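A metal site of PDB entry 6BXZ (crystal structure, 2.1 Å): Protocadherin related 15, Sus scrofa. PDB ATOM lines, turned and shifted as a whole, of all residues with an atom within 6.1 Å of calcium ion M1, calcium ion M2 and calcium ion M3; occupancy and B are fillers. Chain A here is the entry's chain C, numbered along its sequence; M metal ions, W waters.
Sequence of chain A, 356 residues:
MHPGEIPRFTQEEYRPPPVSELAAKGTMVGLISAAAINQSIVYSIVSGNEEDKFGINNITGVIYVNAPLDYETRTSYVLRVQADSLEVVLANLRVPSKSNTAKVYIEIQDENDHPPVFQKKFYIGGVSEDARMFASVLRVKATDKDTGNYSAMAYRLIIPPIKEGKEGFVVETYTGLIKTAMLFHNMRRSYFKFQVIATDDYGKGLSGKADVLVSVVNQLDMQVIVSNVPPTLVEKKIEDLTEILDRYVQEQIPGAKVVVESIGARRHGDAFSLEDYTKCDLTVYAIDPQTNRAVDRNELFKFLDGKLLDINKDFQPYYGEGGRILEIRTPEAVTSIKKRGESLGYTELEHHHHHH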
ATOM      1  N   GLU A  21      -6.418  29.211  32.482  1.00  0.00           N
ATOM      2  CA  GLU A  21      -6.238  30.459  31.735  1.00  0.00           C
ATOM      3  C   GLU A  21      -6.541  31.685  32.590  1.00  0.00           C
ATOM      4  O   GLU A  21      -6.138  32.786  32.210  1.00  0.00           O
ATOM      5  CB  GLU A  21      -7.093  30.494  30.468  1.00  0.00           C
ATOM      6  CG  GLU A  21      -8.591  30.666  30.718  1.00  0.00           C
ATOM      7  CD  GLU A  21      -9.404  30.775  29.430  1.00  0.00           C
ATOM      8  OE1 GLU A  21      -9.225  31.755  28.666  1.00  0.00           O
ATOM      9  OE2 GLU A  21     -10.242  29.877  29.225  1.00  0.00           O
ATOM     10  N   LEU A  22      -7.263  31.510  33.698  1.00  0.00           N
ATOM     11  CA  LEU A  22      -7.502  32.579  34.662  1.00  0.00           C
ATOM     12  C   LEU A  22      -6.492  32.573  35.823  1.00  0.00           C
ATOM     13  O   LEU A  22      -6.739  33.194  36.844  1.00  0.00           O
ATOM     14  CB  LEU A  22      -8.914  32.474  35.249  1.00  0.00           C
ATOM     15  CG  LEU A  22     -10.096  32.375  34.260  1.00  0.00           C
ATOM     16  CD1 LEU A  22     -11.364  31.932  35.001  1.00  0.00           C
ATOM     17  CD2 LEU A  22     -10.336  33.692  33.547  1.00  0.00           C
ATOM     18  N   LEU A  69      -2.945  34.916  31.009  1.00  0.00           N
ATOM     19  CA  LEU A  69      -3.084  33.847  30.012  1.00  0.00           C
ATOM     20  C   LEU A  69      -4.438  33.920  29.310  1.00  0.00           C
ATOM     21  O   LEU A  69      -5.361  34.573  29.779  1.00  0.00           O
ATOM     22  CB  LEU A  69      -2.896  32.482  30.669  1.00  0.00           C
ATOM     23  CG  LEU A  69      -1.513  32.216  31.284  1.00  0.00           C
ATOM     24  CD1 LEU A  69      -1.532  30.926  32.089  1.00  0.00           C
ATOM     25  CD2 LEU A  69      -0.402  32.171  30.242  1.00  0.00           C
ATOM     26  N   ASP A  70      -4.531  33.260  28.171  1.00  0.00           N
ATOM     27  CA  ASP A  70      -5.761  33.221  27.415  1.00  0.00           C
ATOM     28  C   ASP A  70      -5.789  32.005  26.490  1.00  0.00           C
ATOM     29  O   ASP A  70      -5.129  31.985  25.456  1.00  0.00           O
ATOM     30  CB  ASP A  70      -5.927  34.513  26.606  1.00  0.00           C
ATOM     31  CG  ASP A  70      -7.253  34.562  25.844  1.00  0.00           C
ATOM     32  OD1 ASP A  70      -8.233  33.879  26.208  1.00  0.00           O
ATOM     33  OD2 ASP A  70      -7.301  35.304  24.834  1.00  0.00           O
ATOM     34  N   TYR A  71      -6.599  31.028  26.875  1.00  0.00           N
ATOM     35  CA  TYR A  71      -6.801  29.809  26.075  1.00  0.00           C
ATOM     36  C   TYR A  71      -7.238  30.139  24.644  1.00  0.00           C
ATOM     37  O   TYR A  71      -6.822  29.462  23.712  1.00  0.00           O
ATOM     38  CB  TYR A  71      -7.821  28.908  26.763  1.00  0.00           C
ATOM     39  CG  TYR A  71      -8.022  27.597  26.063  1.00  0.00           C
ATOM     40  CD1 TYR A  71      -8.987  27.467  25.054  1.00  0.00           C
ATOM     41  CD2 TYR A  71      -7.260  26.483  26.401  1.00  0.00           C
ATOM     42  CE1 TYR A  71      -9.178  26.257  24.403  1.00  0.00           C
ATOM     43  CE2 TYR A  71      -7.442  25.264  25.755  1.00  0.00           C
ATOM     44  CZ  TYR A  71      -8.391  25.165  24.757  1.00  0.00           C
ATOM     45  OH  TYR A  71      -8.575  23.967  24.117  1.00  0.00           O
ATOM     46  N   GLU A  72      -8.042  31.193  24.503  1.00  0.00           N
ATOM     47  CA  GLU A  72      -8.567  31.594  23.196  1.00  0.00           C
ATOM     48  C   GLU A  72      -7.540  32.264  22.275  1.00  0.00           C
ATOM     49  O   GLU A  72      -7.798  32.415  21.087  1.00  0.00           O
ATOM     50  CB  GLU A  72      -9.820  32.488  23.364  1.00  0.00           C
ATOM     51  CG  GLU A  72     -11.085  31.746  23.784  1.00  0.00           C
ATOM     52  CD  GLU A  72     -11.191  31.394  25.260  1.00  0.00           C
ATOM     53  OE1 GLU A  72     -11.667  30.287  25.632  1.00  0.00           O
ATOM     54  OE2 GLU A  72     -10.838  32.241  26.101  1.00  0.00           O
ATOM     55  N   ASP A 110      -8.837  25.454  29.364  1.00  0.00           N
ATOM     56  CA  ASP A 110      -9.945  26.339  29.028  1.00  0.00           C
ATOM     57  C   ASP A 110     -10.802  26.530  30.282  1.00  0.00           C
ATOM     58  O   ASP A 110     -11.139  25.540  30.933  1.00  0.00           O
ATOM     59  CB  ASP A 110     -10.771  25.733  27.889  1.00  0.00           C
ATOM     60  CG  ASP A 110     -11.930  26.609  27.443  1.00  0.00           C
ATOM     61  OD1 ASP A 110     -11.814  27.863  27.415  1.00  0.00           O
ATOM     62  OD2 ASP A 110     -12.965  26.020  27.080  1.00  0.00           O
ATOM     63  N   GLU A 111     -11.069  27.786  30.632  1.00  0.00           N
ATOM     64  CA  GLU A 111     -12.091  28.129  31.610  1.00  0.00           C
ATOM     65  C   GLU A 111     -13.300  28.789  30.936  1.00  0.00           C
ATOM     66  O   GLU A 111     -13.207  29.293  29.809  1.00  0.00           O
ATOM     67  CB  GLU A 111     -11.573  29.063  32.694  1.00  0.00           C
ATOM     68  CG  GLU A 111     -10.339  28.551  33.456  1.00  0.00           C
ATOM     69  CD  GLU A 111     -10.539  27.258  34.227  1.00  0.00           C
ATOM     70  OE1 GLU A 111     -11.701  26.797  34.404  1.00  0.00           O
ATOM     71  OE2 GLU A 111      -9.507  26.695  34.656  1.00  0.00           O
ATOM     72  N   ASN A 112     -14.400  28.794  31.679  1.00  0.00           N
ATOM     73  CA  ASN A 112     -15.705  29.241  31.180  1.00  0.00           C
ATOM     74  C   ASN A 112     -15.792  30.756  31.359  1.00  0.00           C
ATOM     75  O   ASN A 112     -16.357  31.239  32.338  1.00  0.00           O
ATOM     76  CB  ASN A 112     -16.856  28.522  31.912  1.00  0.00           C
ATOM     77  CG  ASN A 112     -18.196  28.654  31.203  1.00  0.00           C
ATOM     78  OD1 ASN A 112     -18.266  29.175  30.101  1.00  0.00           O
ATOM     79  ND2 ASN A 112     -19.252  28.154  31.837  1.00  0.00           N
ATOM     80  N   ASP A 113     -15.214  31.496  30.414  1.00  0.00           N
ATOM     81  CA  ASP A 113     -15.166  32.958  30.485  1.00  0.00           C
ATOM     82  C   ASP A 113     -15.892  33.665  29.354  1.00  0.00           C
ATOM     83  O   ASP A 113     -15.737  34.868  29.187  1.00  0.00           O
ATOM     84  CB  ASP A 113     -13.712  33.484  30.690  1.00  0.00           C
ATOM     85  CG  ASP A 113     -12.708  33.039  29.605  1.00  0.00           C
ATOM     86  OD1 ASP A 113     -12.999  32.184  28.748  1.00  0.00           O
ATOM     87  OD2 ASP A 113     -11.545  33.555  29.651  1.00  0.00           O
ATOM     88  N   HIS A 114     -16.719  32.952  28.597  1.00  0.00           N
ATOM     89  CA  HIS A 114     -17.547  33.576  27.574  1.00  0.00           C
ATOM     90  C   HIS A 114     -18.968  33.097  27.819  1.00  0.00           C
ATOM     91  O   HIS A 114     -19.206  31.883  27.851  1.00  0.00           O
ATOM     92  CB  HIS A 114     -17.059  33.188  26.170  1.00  0.00           C
ATOM     93  CG  HIS A 114     -15.697  33.694  25.836  1.00  0.00           C
ATOM     94  ND1 HIS A 114     -15.481  34.867  25.133  1.00  0.00           N
ATOM     95  CD2 HIS A 114     -14.471  33.174  26.094  1.00  0.00           C
ATOM     96  CE1 HIS A 114     -14.183  35.051  25.003  1.00  0.00           C
ATOM     97  NE2 HIS A 114     -13.547  34.040  25.551  1.00  0.00           N
ATOM     98  N   PRO A 115     -19.925  34.033  28.007  1.00  0.00           N
ATOM     99  CA  PRO A 115     -21.309  33.570  28.142  1.00  0.00           C
ATOM    100  C   PRO A 115     -21.909  33.209  26.777  1.00  0.00           C
ATOM    101  O   PRO A 115     -21.451  33.719  25.766  1.00  0.00           O
ATOM    102  CB  PRO A 115     -22.022  34.805  28.736  1.00  0.00           C
ATOM    103  CG  PRO A 115     -21.268  35.956  28.175  1.00  0.00           C
ATOM    104  CD  PRO A 115     -19.825  35.509  28.110  1.00  0.00           C
ATOM    105  N   PRO A 116     -22.955  32.361  26.749  1.00  0.00           N
ATOM    106  CA  PRO A 116     -23.707  32.097  25.507  1.00  0.00           C
ATOM    107  C   PRO A 116     -24.232  33.380  24.821  1.00  0.00           C
ATOM    108  O   PRO A 116     -24.697  34.298  25.509  1.00  0.00           O
ATOM    109  CB  PRO A 116     -24.868  31.227  25.991  1.00  0.00           C
ATOM    110  CG  PRO A 116     -24.354  30.568  27.231  1.00  0.00           C
ATOM    111  CD  PRO A 116     -23.534  31.621  27.895  1.00  0.00           C
ATOM    112  N   ASP A 144     -20.630  30.073  22.049  1.00  0.00           N
ATOM    113  CA  ASP A 144     -19.612  30.975  22.589  1.00  0.00           C
ATOM    114  C   ASP A 144     -18.229  30.413  22.289  1.00  0.00           C
ATOM    115  O   ASP A 144     -18.085  29.276  21.869  1.00  0.00           O
ATOM    116  CB  ASP A 144     -19.867  31.379  24.058  1.00  0.00           C
ATOM    117  CG  ASP A 144     -19.694  30.239  25.070  1.00  0.00           C
ATOM    118  OD1 ASP A 144     -18.541  29.839  25.391  1.00  0.00           O
ATOM    119  OD2 ASP A 144     -20.711  29.799  25.662  1.00  0.00           O
ATOM    120  N   LYS A 145     -17.230  31.245  22.524  1.00  0.00           N
ATOM    121  CA  LYS A 145     -15.858  30.939  22.116  1.00  0.00           C
ATOM    122  C   LYS A 145     -15.135  29.900  22.966  1.00  0.00           C
ATOM    123  O   LYS A 145     -14.045  29.476  22.584  1.00  0.00           O
ATOM    124  CB  LYS A 145     -15.008  32.224  22.057  1.00  0.00           C
ATOM    125  CG  LYS A 145     -15.687  33.391  21.353  1.00  0.00           C
ATOM    126  CD  LYS A 145     -14.732  34.383  20.738  1.00  0.00           C
ATOM    127  CE  LYS A 145     -15.538  35.532  20.150  1.00  0.00           C
ATOM    128  NZ  LYS A 145     -14.646  36.604  19.601  1.00  0.00           N
ATOM    129  N   ASP A 146     -15.718  29.451  24.088  1.00  0.00           N
ATOM    130  CA  ASP A 146     -15.105  28.405  24.913  1.00  0.00           C
ATOM    131  C   ASP A 146     -15.191  27.073  24.202  1.00  0.00           C
ATOM    132  O   ASP A 146     -15.891  26.937  23.211  1.00  0.00           O
ATOM    133  CB  ASP A 146     -15.790  28.321  26.284  1.00  0.00           C
ATOM    134  CG  ASP A 146     -15.654  29.600  27.108  1.00  0.00           C
ATOM    135  OD1 ASP A 146     -14.556  30.156  27.127  1.00  0.00           O
ATOM    136  OD2 ASP A 146     -16.627  30.056  27.747  1.00  0.00           O
ATOM    137  N   THR A 147     -14.506  26.066  24.738  1.00  0.00           N
ATOM    138  CA  THR A 147     -14.434  24.744  24.138  1.00  0.00           C
ATOM    139  C   THR A 147     -15.230  23.727  24.941  1.00  0.00           C
ATOM    140  O   THR A 147     -15.478  23.915  26.151  1.00  0.00           O
ATOM    141  CB  THR A 147     -12.966  24.268  24.091  1.00  0.00           C
ATOM    142  OG1 THR A 147     -12.163  25.251  23.423  1.00  0.00           O
ATOM    143  CG2 THR A 147     -12.817  22.910  23.389  1.00  0.00           C
ATOM    144  N   TYR A 150     -17.878  23.879  28.096  1.00  0.00           N
ATOM    145  CA  TYR A 150     -18.025  25.309  28.391  1.00  0.00           C
ATOM    146  C   TYR A 150     -18.690  26.186  27.314  1.00  0.00           C
ATOM    147  O   TYR A 150     -18.926  27.394  27.543  1.00  0.00           O
ATOM    148  CB  TYR A 150     -16.672  25.903  28.849  1.00  0.00           C
ATOM    149  CG  TYR A 150     -16.167  25.364  30.180  1.00  0.00           C
ATOM    150  CD1 TYR A 150     -17.046  24.914  31.182  1.00  0.00           C
ATOM    151  CD2 TYR A 150     -14.792  25.328  30.458  1.00  0.00           C
ATOM    152  CE1 TYR A 150     -16.576  24.446  32.391  1.00  0.00           C
ATOM    153  CE2 TYR A 150     -14.326  24.852  31.678  1.00  0.00           C
ATOM    154  CZ  TYR A 150     -15.220  24.415  32.638  1.00  0.00           C
ATOM    155  OH  TYR A 150     -14.809  23.948  33.832  1.00  0.00           O
ATOM    156  N   SER A 151     -18.991  25.587  26.148  1.00  0.00           N
ATOM    157  CA  SER A 151     -19.901  26.199  25.191  1.00  0.00           C
ATOM    158  C   SER A 151     -21.017  25.228  24.725  1.00  0.00           C
ATOM    159  O   SER A 151     -21.584  25.427  23.670  1.00  0.00           O
ATOM    160  CB  SER A 151     -19.120  26.708  23.987  1.00  0.00           C
ATOM    161  OG  SER A 151     -18.501  25.621  23.328  1.00  0.00           O
ATOM    162  N   MET A 153     -24.668  23.847  25.204  1.00  0.00           N
ATOM    163  CA  MET A 153     -25.826  24.575  25.709  1.00  0.00           C
ATOM    164  C   MET A 153     -26.951  23.686  26.213  1.00  0.00           C
ATOM    165  O   MET A 153     -27.241  22.666  25.608  1.00  0.00           O
ATOM    166  CB  MET A 153     -26.380  25.454  24.579  1.00  0.00           C
ATOM    167  CG  MET A 153     -25.379  26.442  24.008  1.00  0.00           C
ATOM    168  SD  MET A 153     -24.697  27.541  25.260  1.00  0.00           S
ATOM    169  CE  MET A 153     -23.362  28.334  24.356  1.00  0.00           C
ATOM    170  N   ASP A 200     -24.551  27.442  29.323  1.00  0.00           N
ATOM    171  CA  ASP A 200     -23.471  26.526  28.928  1.00  0.00           C
ATOM    172  C   ASP A 200     -23.124  25.576  30.084  1.00  0.00           C
ATOM    173  O   ASP A 200     -23.701  25.643  31.177  1.00  0.00           O
ATOM    174  CB  ASP A 200     -22.254  27.290  28.393  1.00  0.00           C
ATOM    175  CG  ASP A 200     -21.669  28.255  29.398  1.00  0.00           C
ATOM    176  OD1 ASP A 200     -21.741  28.003  30.620  1.00  0.00           O
ATOM    177  OD2 ASP A 200     -21.165  29.306  28.962  1.00  0.00           O
ATOM    178  N   LEU A 206     -22.689  29.699  32.512  1.00  0.00           N
ATOM    179  CA  LEU A 206     -23.114  31.063  32.220  1.00  0.00           C
ATOM    180  C   LEU A 206     -24.314  31.054  31.269  1.00  0.00           C
ATOM    181  O   LEU A 206     -24.532  30.088  30.549  1.00  0.00           O
ATOM    182  CB  LEU A 206     -21.966  31.854  31.592  1.00  0.00           C
ATOM    183  CG  LEU A 206     -20.642  31.975  32.381  1.00  0.00           C
ATOM    184  CD1 LEU A 206     -19.569  32.670  31.552  1.00  0.00           C
ATOM    185  CD2 LEU A 206     -20.854  32.703  33.693  1.00  0.00           C
HETATM  186 CA    CA M   1     -12.295  30.036  27.826  1.00  0.00          CA
HETATM  187 CA    CA M   2     -10.034  33.745  27.736  1.00  0.00          CA
HETATM  188 CA    CA M   3     -19.090  29.625  27.902  1.00  0.00          CA
HETATM  189  O   HOH W   1      -8.640  34.926  29.404  1.00  0.00           O
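Calcium ion M2 is bound by the side-chain carboxylate of Glu 21, the side-chain carboxylate of Glu 72, the side-chain carboxylate of Asp 70, the side-chain carboxylate of Asp 113 and water W1.
The side-chain carboxylate (OE1) of Glu 21 sits close to the backbone NH (N) of Tyr 71. N of Leu 206 lies within hydrogen-bond range of OD1 of Asp 200, at 2.7 Å. O of Asp 146 is in hydrogen-bond range of OG of Ser 151 (2.9 Å). A ring nitrogen (NE2) of His 114 lies close to the side-chain carboxylate (OE2) of Glu 72, at 3.3 Å. OD2 of Asp 110 is in hydrogen-bond range of N of Thr 147, at 2.8 Å.
Calcium ion M3 is bound by the backbone carbonyl oxygen (O) of His 114 (2.3 Å), the backbone carbonyl oxygen (O) of Tyr 150 (2.3 Å), the side-chain carboxylate (OD2) of Asp 200 (2.4 Å), the side-chain amide oxygen (OD1) of Asn 112 (2.4 Å), the side-chain carboxylate (OD2) of Asp 146 (2.5 Å), the side-chain carboxylate (OD1) of Asp 144 (2.6 Å) and the side-chain carboxylate (OD2) of Asp 144 (2.8 Å). Calcium ion M3 has seven donor atoms within binding distance.
The nearest printed residue that does not touch calcium ion M3 is Ser 151 (4.4 Å).
Of the 22 residues printed, 6 come within 4 Å of calcium ion M1. The nearest printed residue that does not touch calcium ion M1 is His 114 (4.2 Å).
Calcium ion M1 is bound by OD1 of Asp 110, OE1 of Glu 72, O of Glu 111, OD1 of Asp 146, OD1 of Asp 113 and OE2 of Glu 21.
Of the 22 residues printed, 4 come within 4 Å of calcium ion M2. The nearest printed residue that does not touch calcium ion M2 is His 114 (4.1 Å).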
